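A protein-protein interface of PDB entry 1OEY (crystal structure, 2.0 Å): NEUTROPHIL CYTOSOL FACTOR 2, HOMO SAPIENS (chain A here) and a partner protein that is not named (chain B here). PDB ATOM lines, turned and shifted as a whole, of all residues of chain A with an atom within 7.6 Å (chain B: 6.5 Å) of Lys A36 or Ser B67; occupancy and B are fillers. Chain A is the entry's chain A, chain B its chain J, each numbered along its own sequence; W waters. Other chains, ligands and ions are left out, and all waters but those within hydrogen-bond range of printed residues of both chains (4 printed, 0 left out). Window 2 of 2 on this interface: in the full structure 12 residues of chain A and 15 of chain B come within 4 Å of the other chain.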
ATOM      1  N   VAL A  10      24.520  -2.747  -9.510  1.00  0.00           N
ATOM      2  CA  VAL A  10      25.157  -1.551 -10.046  1.00  0.00           C
ATOM      3  C   VAL A  10      26.628  -1.768 -10.240  1.00  0.00           C
ATOM      4  O   VAL A  10      27.326  -2.087  -9.308  1.00  0.00           O
ATOM      5  CB  VAL A  10      24.977  -0.309  -9.140  1.00  0.00           C
ATOM      6  CG1 VAL A  10      25.595   0.889  -9.805  1.00  0.00           C
ATOM      7  CG2 VAL A  10      23.492  -0.054  -8.847  1.00  0.00           C
ATOM      8  N   TYR A  14      33.595  -0.831  -8.573  1.00  0.00           N
ATOM      9  CA  TYR A  14      33.211  -2.140  -8.019  1.00  0.00           C
ATOM     10  C   TYR A  14      31.714  -2.338  -8.224  1.00  0.00           C
ATOM     11  O   TYR A  14      30.998  -1.408  -8.606  1.00  0.00           O
ATOM     12  CB  TYR A  14      33.560  -2.233  -6.509  1.00  0.00           C
ATOM     13  CG  TYR A  14      33.056  -1.080  -5.656  1.00  0.00           C
ATOM     14  CD1 TYR A  14      31.815  -1.123  -5.073  1.00  0.00           C
ATOM     15  CD2 TYR A  14      33.827   0.074  -5.466  1.00  0.00           C
ATOM     16  CE1 TYR A  14      31.342  -0.061  -4.284  1.00  0.00           C
ATOM     17  CE2 TYR A  14      33.356   1.163  -4.681  1.00  0.00           C
ATOM     18  CZ  TYR A  14      32.107   1.065  -4.095  1.00  0.00           C
ATOM     19  OH  TYR A  14      31.594   2.085  -3.338  1.00  0.00           O
ATOM     20  N   VAL A  16      27.924  -3.586  -6.734  1.00  0.00           N
ATOM     21  CA  VAL A  16      27.105  -3.729  -5.536  1.00  0.00           C
ATOM     22  C   VAL A  16      25.756  -4.260  -5.930  1.00  0.00           C
ATOM     23  O   VAL A  16      25.361  -4.210  -7.098  1.00  0.00           O
ATOM     24  CB  VAL A  16      26.921  -2.392  -4.737  1.00  0.00           C
ATOM     25  CG1 VAL A  16      28.247  -1.898  -4.282  1.00  0.00           C
ATOM     26  CG2 VAL A  16      26.231  -1.307  -5.559  1.00  0.00           C
ATOM     27  N   VAL A  17      25.064  -4.802  -4.943  1.00  0.00           N
ATOM     28  CA  VAL A  17      23.713  -5.325  -5.121  1.00  0.00           C
ATOM     29  C   VAL A  17      22.862  -4.868  -3.939  1.00  0.00           C
ATOM     30  O   VAL A  17      23.278  -4.963  -2.787  1.00  0.00           O
ATOM     31  CB  VAL A  17      23.717  -6.878  -5.242  1.00  0.00           C
ATOM     32  CG1 VAL A  17      22.277  -7.441  -5.217  1.00  0.00           C
ATOM     33  CG2 VAL A  17      24.403  -7.334  -6.537  1.00  0.00           C
ATOM     34  N   MET A  18      21.678  -4.352  -4.224  1.00  0.00           N
ATOM     35  CA  MET A  18      20.761  -3.910  -3.174  1.00  0.00           C
ATOM     36  C   MET A  18      19.327  -4.257  -3.497  1.00  0.00           C
ATOM     37  O   MET A  18      18.917  -4.353  -4.650  1.00  0.00           O
ATOM     38  CB  MET A  18      20.901  -2.405  -2.917  1.00  0.00           C
ATOM     39  CG  MET A  18      20.220  -1.509  -3.928  1.00  0.00           C
ATOM     40  SD  MET A  18      21.194   0.269  -4.183  1.00  0.00           S
ATOM     41  CE  MET A  18      22.743  -0.435  -5.178  1.00  0.00           C
ATOM     42  N   LYS A  19      18.548  -4.445  -2.446  1.00  0.00           N
ATOM     43  CA  LYS A  19      17.156  -4.775  -2.605  1.00  0.00           C
ATOM     44  C   LYS A  19      16.478  -3.585  -3.230  1.00  0.00           C
ATOM     45  O   LYS A  19      16.878  -2.441  -3.008  1.00  0.00           O
ATOM     46  CB  LYS A  19      16.553  -5.128  -1.255  1.00  0.00           C
ATOM     47  CG  LYS A  19      17.164  -6.411  -0.702  1.00  0.00           C
ATOM     48  CD  LYS A  19      16.330  -7.027   0.421  1.00  0.00           C
ATOM     49  CE  LYS A  19      17.156  -7.292   1.674  1.00  0.00           C
ATOM     50  NZ  LYS A  19      16.278  -7.772   2.816  1.00  0.00           N
ATOM     51  N   ARG A  30      18.224   6.818  -8.354  1.00  0.00           N
ATOM     52  CA  ARG A  30      19.475   7.579  -8.246  1.00  0.00           C
ATOM     53  C   ARG A  30      19.879   7.788  -6.783  1.00  0.00           C
ATOM     54  O   ARG A  30      21.027   7.645  -6.414  1.00  0.00           O
ATOM     55  CB  ARG A  30      19.384   8.945  -8.956  1.00  0.00           C
ATOM     56  CG  ARG A  30      20.724   9.581  -9.196  1.00  0.00           C
ATOM     57  CD  ARG A  30      20.732  10.884 -10.026  1.00  0.00           C
ATOM     58  NE  ARG A  30      19.608  11.752  -9.699  1.00  0.00           N
ATOM     59  CZ  ARG A  30      19.437  12.996 -10.142  1.00  0.00           C
ATOM     60  NH1 ARG A  30      20.331  13.559 -10.948  1.00  0.00           N
ATOM     61  NH2 ARG A  30      18.355  13.681  -9.765  1.00  0.00           N
ATOM     62  N   ASP A  31      18.916   8.146  -5.951  1.00  0.00           N
ATOM     63  CA  ASP A  31      19.206   8.470  -4.553  1.00  0.00           C
ATOM     64  C   ASP A  31      19.768   7.254  -3.780  1.00  0.00           C
ATOM     65  O   ASP A  31      20.693   7.371  -2.973  1.00  0.00           O
ATOM     66  CB  ASP A  31      17.928   8.962  -3.867  1.00  0.00           C
ATOM     67  CG  ASP A  31      18.151   9.292  -2.413  1.00  0.00           C
ATOM     68  OD1 ASP A  31      18.977  10.188  -2.137  1.00  0.00           O
ATOM     69  OD2 ASP A  31      17.568   8.702  -1.478  1.00  0.00           O
ATOM     70  N   MET A  32      19.181   6.093  -4.021  1.00  0.00           N
ATOM     71  CA  MET A  32      19.608   4.880  -3.336  1.00  0.00           C
ATOM     72  C   MET A  32      20.992   4.437  -3.844  1.00  0.00           C
ATOM     73  O   MET A  32      21.816   3.966  -3.057  1.00  0.00           O
ATOM     74  CB  MET A  32      18.518   3.772  -3.391  1.00  0.00           C
ATOM     75  CG  MET A  32      18.220   3.119  -4.729  1.00  0.00           C
ATOM     76  SD  MET A  32      17.023   1.438  -4.536  1.00  0.00           S
ATOM     77  CE  MET A  32      15.704   2.130  -3.058  1.00  0.00           C
ATOM     78  N   VAL A  33      21.291   4.654  -5.125  1.00  0.00           N
ATOM     79  CA  VAL A  33      22.632   4.312  -5.627  1.00  0.00           C
ATOM     80  C   VAL A  33      23.670   5.285  -5.091  1.00  0.00           C
ATOM     81  O   VAL A  33      24.754   4.898  -4.690  1.00  0.00           O
ATOM     82  CB  VAL A  33      22.679   4.267  -7.154  1.00  0.00           C
ATOM     83  CG1 VAL A  33      24.126   4.073  -7.641  1.00  0.00           C
ATOM     84  CG2 VAL A  33      21.779   3.136  -7.662  1.00  0.00           C
ATOM     85  N   SER A  34      23.326   6.564  -5.066  1.00  0.00           N
ATOM     86  CA  SER A  34      24.199   7.601  -4.502  1.00  0.00           C
ATOM     87  C   SER A  34      24.561   7.304  -3.027  1.00  0.00           C
ATOM     88  O   SER A  34      25.721   7.428  -2.614  1.00  0.00           O
ATOM     89  CB  SER A  34      23.478   8.958  -4.631  1.00  0.00           C
ATOM     90  OG  SER A  34      24.084   9.965  -3.844  1.00  0.00           O
ATOM     91  N   LYS A  35      23.568   6.912  -2.233  1.00  0.00           N
ATOM     92  CA  LYS A  35      23.795   6.582  -0.819  1.00  0.00           C
ATOM     93  C   LYS A  35      24.648   5.320  -0.708  1.00  0.00           C
ATOM     94  O   LYS A  35      25.643   5.302   0.012  1.00  0.00           O
ATOM     95  CB  LYS A  35      22.476   6.436  -0.059  1.00  0.00           C
ATOM     96  CG  LYS A  35      21.828   7.772   0.254  1.00  0.00           C
ATOM     97  CD  LYS A  35      20.389   7.614   0.697  1.00  0.00           C
ATOM     98  CE  LYS A  35      19.804   8.952   1.103  1.00  0.00           C
ATOM     99  NZ  LYS A  35      18.343   8.907   1.097  1.00  0.00           N
ATOM    100  N   LYS A  36      24.294   4.281  -1.445  1.00  0.00           N
ATOM    101  CA  LYS A  36      25.059   3.051  -1.388  1.00  0.00           C
ATOM    102  C   LYS A  36      26.521   3.275  -1.753  1.00  0.00           C
ATOM    103  O   LYS A  36      27.373   2.769  -1.072  1.00  0.00           O
ATOM    104  CB  LYS A  36      24.441   1.974  -2.280  1.00  0.00           C
ATOM    105  CG  LYS A  36      25.024   0.569  -2.108  1.00  0.00           C
ATOM    106  CD  LYS A  36      24.587  -0.062  -0.826  1.00  0.00           C
ATOM    107  CE  LYS A  36      24.929  -1.577  -0.782  1.00  0.00           C
ATOM    108  NZ  LYS A  36      24.542  -2.205   0.557  1.00  0.00           N
ATOM    109  N   LEU A  37      26.808   4.050  -2.799  1.00  0.00           N
ATOM    110  CA  LEU A  37      28.183   4.263  -3.265  1.00  0.00           C
ATOM    111  C   LEU A  37      28.884   5.451  -2.616  1.00  0.00           C
ATOM    112  O   LEU A  37      30.008   5.778  -2.979  1.00  0.00           O
ATOM    113  CB  LEU A  37      28.205   4.440  -4.795  1.00  0.00           C
ATOM    114  CG  LEU A  37      27.625   3.305  -5.659  1.00  0.00           C
ATOM    115  CD1 LEU A  37      27.682   3.650  -7.144  1.00  0.00           C
ATOM    116  CD2 LEU A  37      28.378   2.005  -5.410  1.00  0.00           C
ATOM    117  N   GLU A  38      28.213   6.087  -1.664  1.00  0.00           N
ATOM    118  CA  GLU A  38      28.704   7.299  -0.976  1.00  0.00           C
ATOM    119  C   GLU A  38      29.216   8.334  -1.954  1.00  0.00           C
ATOM    120  O   GLU A  38      30.324   8.841  -1.816  1.00  0.00           O
ATOM    121  CB  GLU A  38      29.768   6.938   0.054  1.00  0.00           C
ATOM    122  CG  GLU A  38      29.250   5.923   1.076  1.00  0.00           C
ATOM    123  CD  GLU A  38      30.273   5.573   2.148  1.00  0.00           C
ATOM    124  OE1 GLU A  38      31.431   6.041   2.068  1.00  0.00           O
ATOM    125  OE2 GLU A  38      29.914   4.818   3.071  1.00  0.00           O
ATOM    126  N   LEU A  39      28.392   8.588  -2.967  1.00  0.00           N
ATOM    127  CA  LEU A  39      28.620   9.586  -4.002  1.00  0.00           C
ATOM    128  C   LEU A  39      27.615  10.718  -3.897  1.00  0.00           C
ATOM    129  O   LEU A  39      26.446  10.476  -3.617  1.00  0.00           O
ATOM    130  CB  LEU A  39      28.417   8.967  -5.379  1.00  0.00           C
ATOM    131  CG  LEU A  39      29.336   7.839  -5.811  1.00  0.00           C
ATOM    132  CD1 LEU A  39      28.931   7.411  -7.212  1.00  0.00           C
ATOM    133  CD2 LEU A  39      30.789   8.284  -5.770  1.00  0.00           C
ATOM    134  N   LEU B  35      29.409  -7.708   9.383  1.00  0.00           N
ATOM    135  CA  LEU B  35      30.486  -7.303   8.497  1.00  0.00           C
ATOM    136  C   LEU B  35      31.743  -6.990   9.283  1.00  0.00           C
ATOM    137  O   LEU B  35      32.814  -7.444   8.940  1.00  0.00           O
ATOM    138  CB  LEU B  35      30.062  -6.081   7.678  1.00  0.00           C
ATOM    139  CG  LEU B  35      31.114  -5.529   6.701  1.00  0.00           C
ATOM    140  CD1 LEU B  35      31.605  -6.586   5.769  1.00  0.00           C
ATOM    141  CD2 LEU B  35      30.522  -4.395   5.895  1.00  0.00           C
ATOM    142  N   ARG B  64      30.837  -6.586  -4.020  1.00  0.00           N
ATOM    143  CA  ARG B  64      31.452  -6.064  -2.815  1.00  0.00           C
ATOM    144  C   ARG B  64      30.409  -5.920  -1.700  1.00  0.00           C
ATOM    145  O   ARG B  64      29.292  -5.441  -1.911  1.00  0.00           O
ATOM    146  CB  ARG B  64      32.154  -4.726  -3.115  1.00  0.00           C
ATOM    147  CG  ARG B  64      32.840  -4.064  -1.906  1.00  0.00           C
ATOM    148  CD  ARG B  64      33.608  -2.810  -2.224  1.00  0.00           C
ATOM    149  NE  ARG B  64      34.771  -3.067  -3.070  1.00  0.00           N
ATOM    150  CZ  ARG B  64      35.805  -2.256  -3.189  1.00  0.00           C
ATOM    151  NH1 ARG B  64      35.805  -1.087  -2.577  1.00  0.00           N
ATOM    152  NH2 ARG B  64      36.825  -2.600  -3.942  1.00  0.00           N
ATOM    153  N   LEU B  65      30.777  -6.395  -0.518  1.00  0.00           N
ATOM    154  CA  LEU B  65      29.957  -6.300   0.676  1.00  0.00           C
ATOM    155  C   LEU B  65      30.208  -4.955   1.323  1.00  0.00           C
ATOM    156  O   LEU B  65      31.356  -4.660   1.653  1.00  0.00           O
ATOM    157  CB  LEU B  65      30.400  -7.385   1.681  1.00  0.00           C
ATOM    158  CG  LEU B  65      30.172  -8.835   1.250  1.00  0.00           C
ATOM    159  CD1 LEU B  65      30.902  -9.782   2.146  1.00  0.00           C
ATOM    160  CD2 LEU B  65      28.659  -9.163   1.345  1.00  0.00           C
ATOM    161  N   LEU B  66      29.154  -4.175   1.572  1.00  0.00           N
ATOM    162  CA  LEU B  66      29.316  -2.865   2.245  1.00  0.00           C
ATOM    163  C   LEU B  66      28.588  -2.697   3.564  1.00  0.00           C
ATOM    164  O   LEU B  66      28.746  -1.699   4.244  1.00  0.00           O
ATOM    165  CB  LEU B  66      28.868  -1.733   1.332  1.00  0.00           C
ATOM    166  CG  LEU B  66      29.617  -1.641   0.012  1.00  0.00           C
ATOM    167  CD1 LEU B  66      29.046  -0.476  -0.791  1.00  0.00           C
ATOM    168  CD2 LEU B  66      31.113  -1.432   0.252  1.00  0.00           C
ATOM    169  N   SER B  67      27.758  -3.648   3.928  1.00  0.00           N
ATOM    170  CA  SER B  67      26.970  -3.497   5.135  1.00  0.00           C
ATOM    171  C   SER B  67      26.550  -4.861   5.633  1.00  0.00           C
ATOM    172  O   SER B  67      26.741  -5.853   4.949  1.00  0.00           O
ATOM    173  CB  SER B  67      25.721  -2.681   4.811  1.00  0.00           C
ATOM    174  OG  SER B  67      24.829  -3.507   4.082  1.00  0.00           O
ATOM    175  N   ASP B  68      25.953  -4.884   6.822  1.00  0.00           N
ATOM    176  CA  ASP B  68      25.466  -6.123   7.423  1.00  0.00           C
ATOM    177  C   ASP B  68      24.392  -6.746   6.554  1.00  0.00           C
ATOM    178  O   ASP B  68      24.337  -7.956   6.417  1.00  0.00           O
ATOM    179  CB  ASP B  68      24.913  -5.876   8.824  1.00  0.00           C
ATOM    180  CG  ASP B  68      25.996  -5.499   9.821  1.00  0.00           C
ATOM    181  OD1 ASP B  68      27.172  -5.898   9.654  1.00  0.00           O
ATOM    182  OD2 ASP B  68      25.751  -4.791  10.806  1.00  0.00           O
ATOM    183  N   GLU B  69      23.565  -5.908   5.938  1.00  0.00           N
ATOM    184  CA  GLU B  69      22.492  -6.386   5.060  1.00  0.00           C
ATOM    185  C   GLU B  69      23.025  -7.069   3.787  1.00  0.00           C
ATOM    186  O   GLU B  69      22.457  -8.067   3.332  1.00  0.00           O
ATOM    187  CB  GLU B  69      21.520  -5.230   4.749  1.00  0.00           C
ATOM    188  CG  GLU B  69      20.545  -5.469   3.596  1.00  0.00           C
ATOM    189  CD  GLU B  69      19.408  -4.436   3.542  1.00  0.00           C
ATOM    190  OE1 GLU B  69      19.391  -3.603   2.593  1.00  0.00           O
ATOM    191  OE2 GLU B  69      18.532  -4.445   4.452  1.00  0.00           O
ATOM    192  N   ASP B  70      24.138  -6.586   3.238  1.00  0.00           N
ATOM    193  CA  ASP B  70      24.789  -7.272   2.117  1.00  0.00           C
ATOM    194  C   ASP B  70      25.283  -8.663   2.508  1.00  0.00           C
ATOM    195  O   ASP B  70      25.120  -9.607   1.757  1.00  0.00           O
ATOM    196  CB  ASP B  70      25.987  -6.469   1.602  1.00  0.00           C
ATOM    197  CG  ASP B  70      25.593  -5.153   0.971  1.00  0.00           C
ATOM    198  OD1 ASP B  70      24.370  -4.872   0.803  1.00  0.00           O
ATOM    199  OD2 ASP B  70      26.443  -4.334   0.586  1.00  0.00           O
ATOM    200  N   VAL B  71      25.898  -8.767   3.687  1.00  0.00           N
ATOM    201  CA  VAL B  71      26.336 -10.030   4.234  1.00  0.00           C
ATOM    202  C   VAL B  71      25.175 -11.018   4.343  1.00  0.00           C
ATOM    203  O   VAL B  71      25.324 -12.161   3.987  1.00  0.00           O
ATOM    204  CB  VAL B  71      27.029  -9.826   5.609  1.00  0.00           C
ATOM    205  CG1 VAL B  71      27.242 -11.127   6.310  1.00  0.00           C
ATOM    206  CG2 VAL B  71      28.384  -9.070   5.445  1.00  0.00           C
ATOM    207  N   ALA B  72      24.027 -10.564   4.817  1.00  0.00           N
ATOM    208  CA  ALA B  72      22.843 -11.409   4.989  1.00  0.00           C
ATOM    209  C   ALA B  72      22.324 -11.924   3.659  1.00  0.00           C
ATOM    210  O   ALA B  72      21.925 -13.065   3.552  1.00  0.00           O
ATOM    211  CB  ALA B  72      21.722 -10.649   5.783  1.00  0.00           C
HETATM  212  O   HOH W   1      19.670  -4.058   0.117  1.00  0.00           O
HETATM  213  O   HOH W   2      22.721  -1.934   3.133  1.00  0.00           O
HETATM  214  O   HOH W   3      26.440  -5.061  -2.466  1.00  0.00           O
HETATM  215  O   HOH W   4      22.465  -6.257  -0.660  1.00  0.00           O
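Water W1 bridges OE1 of Glu B69 and N of Lys A19. Water W4 bridges the backbone carbonyl oxygen (O) of Val A17 and the side-chain carboxylate (OD1) of Asp B70. Water W2 lies within hydrogen-bond range of OG of Ser B67 (2.8 Å) and NZ of Lys A36 (3.2 Å). Water W3 lies within hydrogen-bond range of the backbone NH of Val A17 (2.8 Å), the backbone carbonyl oxygen of Arg B64 (2.9 Å) and the side-chain carboxylate of Asp B70 (3.1 Å).
Printed residues of chain B that touch a printed residue of chain A: Arg B64, Leu B66, Ser B67 and Asp B70. Hydrophobic or aromatic side chains of chain B within 4 Å of the printed part of chain A: Leu B66. Of the 16 printed residues of chain A, 4 touch a printed residue of chain B. Hydrophobic or aromatic side chains of chain A within 4 Å of the printed part of chain B: Tyr A14 and Val A16. Along chain A the printed residues that touch a printed residue of chain B span positions 14 to 36.
Arg B64 touches Tyr A14. CD1 of Leu B66 touches CG1 of Val A16, 3.9 Å away. Asp B70 touches Val A17 (OD1 to O, 3.8 Å). O of Lys A36 touches CD1 of Leu B66 (3.7 Å). Ser B67 touches Lys A36.
The backbone NH (N) of Asp B70 lies within hydrogen-bond range of the side-chain hydroxyl (OG) of Ser B67. N of Leu B66 lies within hydrogen-bond range of OD2 of Asp B70 (2.9 Å). O of Val A16 is in hydrogen-bond range of N of Val A10, at 2.9 Å. The side-chain hydroxyl (OG) of Ser B67 sits close to the backbone NH (N) of Glu B69.
Lys A36 touches three residues of chain B. Ser B67 touches one residue of chain A. Printed residues of chain B within 4 Å of Val A17: Asp B70 (3.8 Å). Printed residues of chain B within 4 Å of Tyr A14: Arg B64 (3.7 Å). Of the printed residues of chain B, Val A16 touches Leu B66 (3.9 Å). Of the printed residues of chain A, Asp B70 touches Val A17 (3.8 Å) and Lys A36 (2.7 Å). Met A32 touches none of the printed residues of chain B. Ser A34 touches none of the printed residues of chain B. The nearest residue of chain A that does not touch Ser B67 is Val A17 (7.2 Å). The nearest printed residue of chain B that does not touch Val A16 is Arg B64 (4.4 Å).
The side-chain amino group (NZ) of Lys A36 lies within salt-bridge range of the side-chain carboxylate (OD1) of Asp B70 (2.7 Å).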
